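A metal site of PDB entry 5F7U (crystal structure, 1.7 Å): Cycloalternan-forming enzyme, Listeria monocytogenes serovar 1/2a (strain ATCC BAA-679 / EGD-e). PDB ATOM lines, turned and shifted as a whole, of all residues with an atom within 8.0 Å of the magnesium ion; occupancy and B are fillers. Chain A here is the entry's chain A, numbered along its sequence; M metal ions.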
ATOM      1  N   THR A 913     -17.441 -23.064 -13.717  1.00  0.00           N
ATOM      2  CA  THR A 913     -17.748 -21.907 -12.848  1.00  0.00           C
ATOM      3  C   THR A 913     -18.895 -22.148 -11.844  1.00  0.00           C
ATOM      4  O   THR A 913     -18.985 -21.456 -10.819  1.00  0.00           O
ATOM      5  CB  THR A 913     -18.060 -20.627 -13.663  1.00  0.00           C
ATOM      6  OG1 THR A 913     -19.311 -20.774 -14.312  1.00  0.00           O
ATOM      7  CG2 THR A 913     -16.982 -20.358 -14.707  1.00  0.00           C
ATOM      8  N   VAL A 914     -19.779 -23.101 -12.154  1.00  0.00           N
ATOM      9  CA  VAL A 914     -20.946 -23.396 -11.305  1.00  0.00           C
ATOM     10  C   VAL A 914     -20.513 -24.153 -10.055  1.00  0.00           C
ATOM     11  O   VAL A 914     -20.979 -23.849  -8.953  1.00  0.00           O
ATOM     12  CB  VAL A 914     -22.049 -24.182 -12.069  1.00  0.00           C
ATOM     13  CG1 VAL A 914     -23.167 -24.657 -11.148  1.00  0.00           C
ATOM     14  CG2 VAL A 914     -22.635 -23.295 -13.155  1.00  0.00           C
ATOM     15  N   ASN A 916     -17.163 -24.515  -9.198  1.00  0.00           N
ATOM     16  CA  ASN A 916     -15.808 -24.076  -8.832  1.00  0.00           C
ATOM     17  C   ASN A 916     -14.817 -25.238  -8.834  1.00  0.00           C
ATOM     18  O   ASN A 916     -14.080 -25.474  -7.877  1.00  0.00           O
ATOM     19  CB  ASN A 916     -15.829 -23.300  -7.514  1.00  0.00           C
ATOM     20  CG  ASN A 916     -16.624 -22.016  -7.607  1.00  0.00           C
ATOM     21  OD1 ASN A 916     -16.357 -21.156  -8.460  1.00  0.00           O
ATOM     22  ND2 ASN A 916     -17.612 -21.874  -6.729  1.00  0.00           N
ATOM     23  N   PRO A 940     -14.261 -20.166  -4.140  1.00  0.00           N
ATOM     24  CA  PRO A 940     -15.011 -19.061  -3.540  1.00  0.00           C
ATOM     25  C   PRO A 940     -16.061 -19.542  -2.534  1.00  0.00           C
ATOM     26  O   PRO A 940     -16.538 -20.683  -2.612  1.00  0.00           O
ATOM     27  CB  PRO A 940     -15.736 -18.424  -4.735  1.00  0.00           C
ATOM     28  CG  PRO A 940     -14.913 -18.817  -5.920  1.00  0.00           C
ATOM     29  CD  PRO A 940     -14.419 -20.187  -5.604  1.00  0.00           C
ATOM     30  N   TYR A 941     -16.375 -18.654  -1.576  1.00  0.00           N
ATOM     31  CA  TYR A 941     -17.546 -18.772  -0.727  1.00  0.00           C
ATOM     32  C   TYR A 941     -18.668 -18.006  -1.430  1.00  0.00           C
ATOM     33  O   TYR A 941     -18.633 -16.771  -1.497  1.00  0.00           O
ATOM     34  CB  TYR A 941     -17.263 -18.143   0.649  1.00  0.00           C
ATOM     35  CG  TYR A 941     -16.276 -18.933   1.474  1.00  0.00           C
ATOM     36  CD1 TYR A 941     -14.888 -18.807   1.274  1.00  0.00           C
ATOM     37  CD2 TYR A 941     -16.731 -19.824   2.453  1.00  0.00           C
ATOM     38  CE1 TYR A 941     -13.988 -19.556   2.031  1.00  0.00           C
ATOM     39  CE2 TYR A 941     -15.843 -20.543   3.228  1.00  0.00           C
ATOM     40  CZ  TYR A 941     -14.477 -20.427   3.000  1.00  0.00           C
ATOM     41  OH  TYR A 941     -13.621 -21.175   3.782  1.00  0.00           O
ATOM     42  N   GLU A 942     -19.651 -18.731  -1.955  1.00  0.00           N
ATOM     43  CA  GLU A 942     -20.694 -18.111  -2.772  1.00  0.00           C
ATOM     44  C   GLU A 942     -21.671 -17.334  -1.912  1.00  0.00           C
ATOM     45  O   GLU A 942     -22.179 -17.845  -0.886  1.00  0.00           O
ATOM     46  CB  GLU A 942     -21.437 -19.162  -3.620  1.00  0.00           C
ATOM     47  CG  GLU A 942     -20.566 -19.849  -4.671  1.00  0.00           C
ATOM     48  CD  GLU A 942     -19.970 -18.892  -5.703  1.00  0.00           C
ATOM     49  OE1 GLU A 942     -20.525 -17.781  -5.931  1.00  0.00           O
ATOM     50  OE2 GLU A 942     -18.948 -19.284  -6.313  1.00  0.00           O
ATOM     51  N   ALA A 943     -21.934 -16.080  -2.308  1.00  0.00           N
ATOM     52  CA  ALA A 943     -22.851 -15.242  -1.560  1.00  0.00           C
ATOM     53  C   ALA A 943     -24.259 -15.841  -1.511  1.00  0.00           C
ATOM     54  O   ALA A 943     -24.956 -15.728  -0.497  1.00  0.00           O
ATOM     55  CB  ALA A 943     -22.877 -13.820  -2.131  1.00  0.00           C
ATOM     56  N   GLU A 944     -24.658 -16.514  -2.593  1.00  0.00           N
ATOM     57  CA  GLU A 944     -25.981 -17.133  -2.701  1.00  0.00           C
ATOM     58  C   GLU A 944     -26.175 -18.320  -1.737  1.00  0.00           C
ATOM     59  O   GLU A 944     -27.315 -18.747  -1.479  1.00  0.00           O
ATOM     60  CB  GLU A 944     -26.271 -17.538  -4.168  1.00  0.00           C
ATOM     61  CG  GLU A 944     -25.284 -18.522  -4.793  1.00  0.00           C
ATOM     62  CD  GLU A 944     -24.126 -17.888  -5.577  1.00  0.00           C
ATOM     63  OE1 GLU A 944     -23.624 -16.779  -5.290  1.00  0.00           O
ATOM     64  OE2 GLU A 944     -23.679 -18.548  -6.523  1.00  0.00           O
ATOM     65  N   PHE A 945     -25.058 -18.837  -1.201  1.00  0.00           N
ATOM     66  CA  PHE A 945     -25.098 -19.891  -0.169  1.00  0.00           C
ATOM     67  C   PHE A 945     -24.977 -19.350   1.251  1.00  0.00           C
ATOM     68  O   PHE A 945     -25.035 -20.116   2.236  1.00  0.00           O
ATOM     69  CB  PHE A 945     -24.019 -20.964  -0.402  1.00  0.00           C
ATOM     70  CG  PHE A 945     -24.055 -21.633  -1.755  1.00  0.00           C
ATOM     71  CD1 PHE A 945     -25.242 -21.748  -2.513  1.00  0.00           C
ATOM     72  CD2 PHE A 945     -22.889 -22.202  -2.275  1.00  0.00           C
ATOM     73  CE1 PHE A 945     -25.243 -22.385  -3.760  1.00  0.00           C
ATOM     74  CE2 PHE A 945     -22.880 -22.837  -3.515  1.00  0.00           C
ATOM     75  CZ  PHE A 945     -24.060 -22.936  -4.263  1.00  0.00           C
ATOM     76  N   ALA A 954     -30.333 -13.792  -7.367  1.00  0.00           N
ATOM     77  CA  ALA A 954     -30.677 -13.701  -8.789  1.00  0.00           C
ATOM     78  C   ALA A 954     -29.567 -14.288  -9.677  1.00  0.00           C
ATOM     79  O   ALA A 954     -28.477 -14.635  -9.193  1.00  0.00           O
ATOM     80  CB  ALA A 954     -31.002 -12.264  -9.178  1.00  0.00           C
ATOM     81  N   GLY A 959     -21.858 -14.165 -15.843  1.00  0.00           N
ATOM     82  CA  GLY A 959     -20.453 -14.079 -15.428  1.00  0.00           C
ATOM     83  C   GLY A 959     -20.154 -14.394 -13.979  1.00  0.00           C
ATOM     84  O   GLY A 959     -18.998 -14.418 -13.590  1.00  0.00           O
ATOM     85  N   TYR A 960     -21.203 -14.617 -13.180  1.00  0.00           N
ATOM     86  CA  TYR A 960     -21.069 -14.989 -11.775  1.00  0.00           C
ATOM     87  C   TYR A 960     -20.497 -16.395 -11.626  1.00  0.00           C
ATOM     88  O   TYR A 960     -20.556 -17.205 -12.551  1.00  0.00           O
ATOM     89  CB  TYR A 960     -22.439 -14.948 -11.068  1.00  0.00           C
ATOM     90  CG  TYR A 960     -23.499 -15.774 -11.776  1.00  0.00           C
ATOM     91  CD1 TYR A 960     -23.578 -17.171 -11.607  1.00  0.00           C
ATOM     92  CD2 TYR A 960     -24.410 -15.161 -12.645  1.00  0.00           C
ATOM     93  CE1 TYR A 960     -24.530 -17.922 -12.285  1.00  0.00           C
ATOM     94  CE2 TYR A 960     -25.379 -15.902 -13.328  1.00  0.00           C
ATOM     95  CZ  TYR A 960     -25.437 -17.272 -13.136  1.00  0.00           C
ATOM     96  OH  TYR A 960     -26.399 -18.014 -13.803  1.00  0.00           O
ATOM     97  N   THR A 961     -19.965 -16.678 -10.449  1.00  0.00           N
ATOM     98  CA  THR A 961     -19.611 -18.037 -10.083  1.00  0.00           C
ATOM     99  C   THR A 961     -20.740 -18.594  -9.203  1.00  0.00           C
ATOM    100  O   THR A 961     -21.573 -17.825  -8.633  1.00  0.00           O
ATOM    101  CB  THR A 961     -18.239 -18.123  -9.381  1.00  0.00           C
ATOM    102  OG1 THR A 961     -18.308 -17.478  -8.121  1.00  0.00           O
ATOM    103  CG2 THR A 961     -17.111 -17.500 -10.246  1.00  0.00           C
ATOM    104  N   GLY A 962     -20.737 -19.919  -9.080  1.00  0.00           N
ATOM    105  CA  GLY A 962     -21.800 -20.642  -8.391  1.00  0.00           C
ATOM    106  C   GLY A 962     -23.076 -20.601  -9.219  1.00  0.00           C
ATOM    107  O   GLY A 962     -23.012 -20.596 -10.450  1.00  0.00           O
ATOM    108  N   THR A 963     -24.222 -20.548  -8.552  1.00  0.00           N
ATOM    109  CA  THR A 963     -25.517 -20.527  -9.240  1.00  0.00           C
ATOM    110  C   THR A 963     -26.094 -19.130  -9.469  1.00  0.00           C
ATOM    111  O   THR A 963     -27.132 -18.989 -10.133  1.00  0.00           O
ATOM    112  CB  THR A 963     -26.564 -21.375  -8.486  1.00  0.00           C
ATOM    113  OG1 THR A 963     -26.771 -20.833  -7.175  1.00  0.00           O
ATOM    114  CG2 THR A 963     -26.131 -22.845  -8.404  1.00  0.00           C
ATOM    115  N   GLY A 964     -25.439 -18.116  -8.918  1.00  0.00           N
ATOM    116  CA  GLY A 964     -25.887 -16.723  -9.065  1.00  0.00           C
ATOM    117  C   GLY A 964     -25.165 -15.766  -8.135  1.00  0.00           C
ATOM    118  O   GLY A 964     -23.936 -15.879  -7.926  1.00  0.00           O
ATOM    119  N   PHE A 965     -25.944 -14.839  -7.590  1.00  0.00           N
ATOM    120  CA  PHE A 965     -25.462 -13.743  -6.747  1.00  0.00           C
ATOM    121  C   PHE A 965     -26.592 -13.233  -5.866  1.00  0.00           C
ATOM    122  O   PHE A 965     -27.768 -13.488  -6.140  1.00  0.00           O
ATOM    123  CB  PHE A 965     -24.891 -12.604  -7.618  1.00  0.00           C
ATOM    124  CG  PHE A 965     -25.809 -12.146  -8.728  1.00  0.00           C
ATOM    125  CD1 PHE A 965     -26.816 -11.204  -8.474  1.00  0.00           C
ATOM    126  CD2 PHE A 965     -25.647 -12.638 -10.030  1.00  0.00           C
ATOM    127  CE1 PHE A 965     -27.638 -10.764  -9.501  1.00  0.00           C
ATOM    128  CE2 PHE A 965     -26.501 -12.210 -11.056  1.00  0.00           C
ATOM    129  CZ  PHE A 965     -27.488 -11.270 -10.792  1.00  0.00           C
ATOM    130  N   VAL A 966     -26.227 -12.494  -4.824  1.00  0.00           N
ATOM    131  CA  VAL A 966     -27.191 -11.781  -3.972  1.00  0.00           C
ATOM    132  C   VAL A 966     -27.485 -10.442  -4.654  1.00  0.00           C
ATOM    133  O   VAL A 966     -26.555  -9.702  -4.994  1.00  0.00           O
ATOM    134  CB  VAL A 966     -26.623 -11.620  -2.551  1.00  0.00           C
ATOM    135  CG1 VAL A 966     -27.461 -10.649  -1.727  1.00  0.00           C
ATOM    136  CG2 VAL A 966     -26.568 -12.970  -1.859  1.00  0.00           C
ATOM    137  N   ARG A 994     -16.220 -10.037  -4.853  1.00  0.00           N
ATOM    138  CA  ARG A 994     -16.621  -9.928  -6.250  1.00  0.00           C
ATOM    139  C   ARG A 994     -18.076  -9.494  -6.351  1.00  0.00           C
ATOM    140  O   ARG A 994     -18.967 -10.127  -5.810  1.00  0.00           O
ATOM    141  CB  ARG A 994     -16.373 -11.237  -7.021  1.00  0.00           C
ATOM    142  CG  ARG A 994     -16.579 -11.097  -8.528  1.00  0.00           C
ATOM    143  CD  ARG A 994     -16.003 -12.277  -9.294  1.00  0.00           C
ATOM    144  NE  ARG A 994     -15.940 -12.041 -10.746  1.00  0.00           N
ATOM    145  CZ  ARG A 994     -16.738 -12.607 -11.650  1.00  0.00           C
ATOM    146  NH1 ARG A 994     -17.703 -13.458 -11.291  1.00  0.00           N
ATOM    147  NH2 ARG A 994     -16.559 -12.320 -12.942  1.00  0.00           N
ATOM    148  N   TRP A1026     -18.380  -7.374 -13.712  1.00  0.00           N
ATOM    149  CA  TRP A1026     -17.981  -7.726 -12.346  1.00  0.00           C
ATOM    150  C   TRP A1026     -16.616  -7.132 -12.031  1.00  0.00           C
ATOM    151  O   TRP A1026     -15.786  -6.962 -12.924  1.00  0.00           O
ATOM    152  CB  TRP A1026     -17.944  -9.254 -12.144  1.00  0.00           C
ATOM    153  CG  TRP A1026     -19.252  -9.927 -12.449  1.00  0.00           C
ATOM    154  CD1 TRP A1026     -19.629 -10.494 -13.632  1.00  0.00           C
ATOM    155  CD2 TRP A1026     -20.370 -10.095 -11.556  1.00  0.00           C
ATOM    156  NE1 TRP A1026     -20.910 -10.999 -13.534  1.00  0.00           N
ATOM    157  CE2 TRP A1026     -21.385 -10.770 -12.273  1.00  0.00           C
ATOM    158  CE3 TRP A1026     -20.608  -9.735 -10.218  1.00  0.00           C
ATOM    159  CZ2 TRP A1026     -22.631 -11.094 -11.700  1.00  0.00           C
ATOM    160  CZ3 TRP A1026     -21.843 -10.056  -9.637  1.00  0.00           C
ATOM    161  CH2 TRP A1026     -22.843 -10.725 -10.392  1.00  0.00           C
ATOM    162  N   PHE A1056     -23.877  -9.153  -5.481  1.00  0.00           N
ATOM    163  CA  PHE A1056     -22.772  -9.698  -4.682  1.00  0.00           C
ATOM    164  C   PHE A1056     -22.572 -11.168  -5.059  1.00  0.00           C
ATOM    165  O   PHE A1056     -23.402 -12.017  -4.747  1.00  0.00           O
ATOM    166  CB  PHE A1056     -23.117  -9.463  -3.200  1.00  0.00           C
ATOM    167  CG  PHE A1056     -22.054  -9.872  -2.196  1.00  0.00           C
ATOM    168  CD1 PHE A1056     -20.730 -10.157  -2.556  1.00  0.00           C
ATOM    169  CD2 PHE A1056     -22.393  -9.911  -0.838  1.00  0.00           C
ATOM    170  CE1 PHE A1056     -19.783 -10.513  -1.582  1.00  0.00           C
ATOM    171  CE2 PHE A1056     -21.466 -10.261   0.139  1.00  0.00           C
ATOM    172  CZ  PHE A1056     -20.154 -10.549  -0.229  1.00  0.00           C
ATOM    173  N   ASP A1057     -21.482 -11.457  -5.771  1.00  0.00           N
ATOM    174  CA  ASP A1057     -21.239 -12.799  -6.315  1.00  0.00           C
ATOM    175  C   ASP A1057     -20.682 -13.802  -5.283  1.00  0.00           C
ATOM    176  O   ASP A1057     -21.258 -14.857  -5.063  1.00  0.00           O
ATOM    177  CB  ASP A1057     -20.291 -12.729  -7.515  1.00  0.00           C
ATOM    178  CG  ASP A1057     -20.145 -14.075  -8.224  1.00  0.00           C
ATOM    179  OD1 ASP A1057     -20.971 -15.004  -8.005  1.00  0.00           O
ATOM    180  OD2 ASP A1057     -19.187 -14.183  -9.019  1.00  0.00           O
ATOM    181  N   HIS A1058     -19.550 -13.458  -4.690  1.00  0.00           N
ATOM    182  CA  HIS A1058     -18.795 -14.379  -3.831  1.00  0.00           C
ATOM    183  C   HIS A1058     -17.698 -13.643  -3.104  1.00  0.00           C
ATOM    184  O   HIS A1058     -17.407 -12.493  -3.430  1.00  0.00           O
ATOM    185  CB  HIS A1058     -18.183 -15.547  -4.657  1.00  0.00           C
ATOM    186  CG  HIS A1058     -17.037 -15.173  -5.557  1.00  0.00           C
ATOM    187  ND1 HIS A1058     -16.922 -15.655  -6.845  1.00  0.00           N
ATOM    188  CD2 HIS A1058     -15.915 -14.432  -5.338  1.00  0.00           C
ATOM    189  CE1 HIS A1058     -15.788 -15.220  -7.384  1.00  0.00           C
ATOM    190  NE2 HIS A1058     -15.165 -14.471  -6.500  1.00  0.00           N
ATOM    191  N   VAL A1059     -17.101 -14.319  -2.118  1.00  0.00           N
ATOM    192  CA  VAL A1059     -15.809 -13.910  -1.568  1.00  0.00           C
ATOM    193  C   VAL A1059     -14.765 -15.016  -1.748  1.00  0.00           C
ATOM    194  O   VAL A1059     -15.102 -16.203  -1.744  1.00  0.00           O
ATOM    195  CB  VAL A1059     -15.891 -13.432  -0.080  1.00  0.00           C
ATOM    196  CG1 VAL A1059     -16.852 -12.242   0.073  1.00  0.00           C
ATOM    197  CG2 VAL A1059     -16.284 -14.561   0.858  1.00  0.00           C
HETATM  198 MG    MG M   1     -22.102 -16.560  -6.901  1.00  0.00          MG
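The magnesium ion is bound by O of Gly 964 (2.2 Å), O of Thr 961 (2.2 Å), OD1 of Asp 1057 (2.2 Å), OE1 of Glu 942 (2.2 Å), OE1 of Glu 944 (2.2 Å) and OE2 of Glu 944 (2.6 Å). Slightly farther from the magnesium ion lies O of Asp 1057 (2.6 Å).
Of the 24 residues printed, 5 come within 4 Å of the magnesium ion.
OG1 of Thr 961 is in hydrogen-bond range of ND1 of His 1058 (2.6 Å). The side-chain carboxylate (OD2) of Asp 1057 is in hydrogen-bond range of a ring nitrogen (ND1) of His 1058 (3.5 Å). The backbone carbonyl oxygen (O) of Asp 1057 is in hydrogen-bond range of the backbone NH (N) of Ala 943 (3.1 Å). The side-chain carboxylate of Asp 1057 is in salt-bridge range of the guanidinium group of Arg 994 (2.8 Å). OE2 of Glu 942 is in hydrogen-bond range of N of Gly 962 (3.4 Å). The side-chain amide nitrogen (ND2) of Asn 916 is in hydrogen-bond range of the side-chain carboxylate (OE2) of Glu 942. The side-chain carboxylate of Glu 944 sits close to the backbone NH of Thr 963 (2.9 Å).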
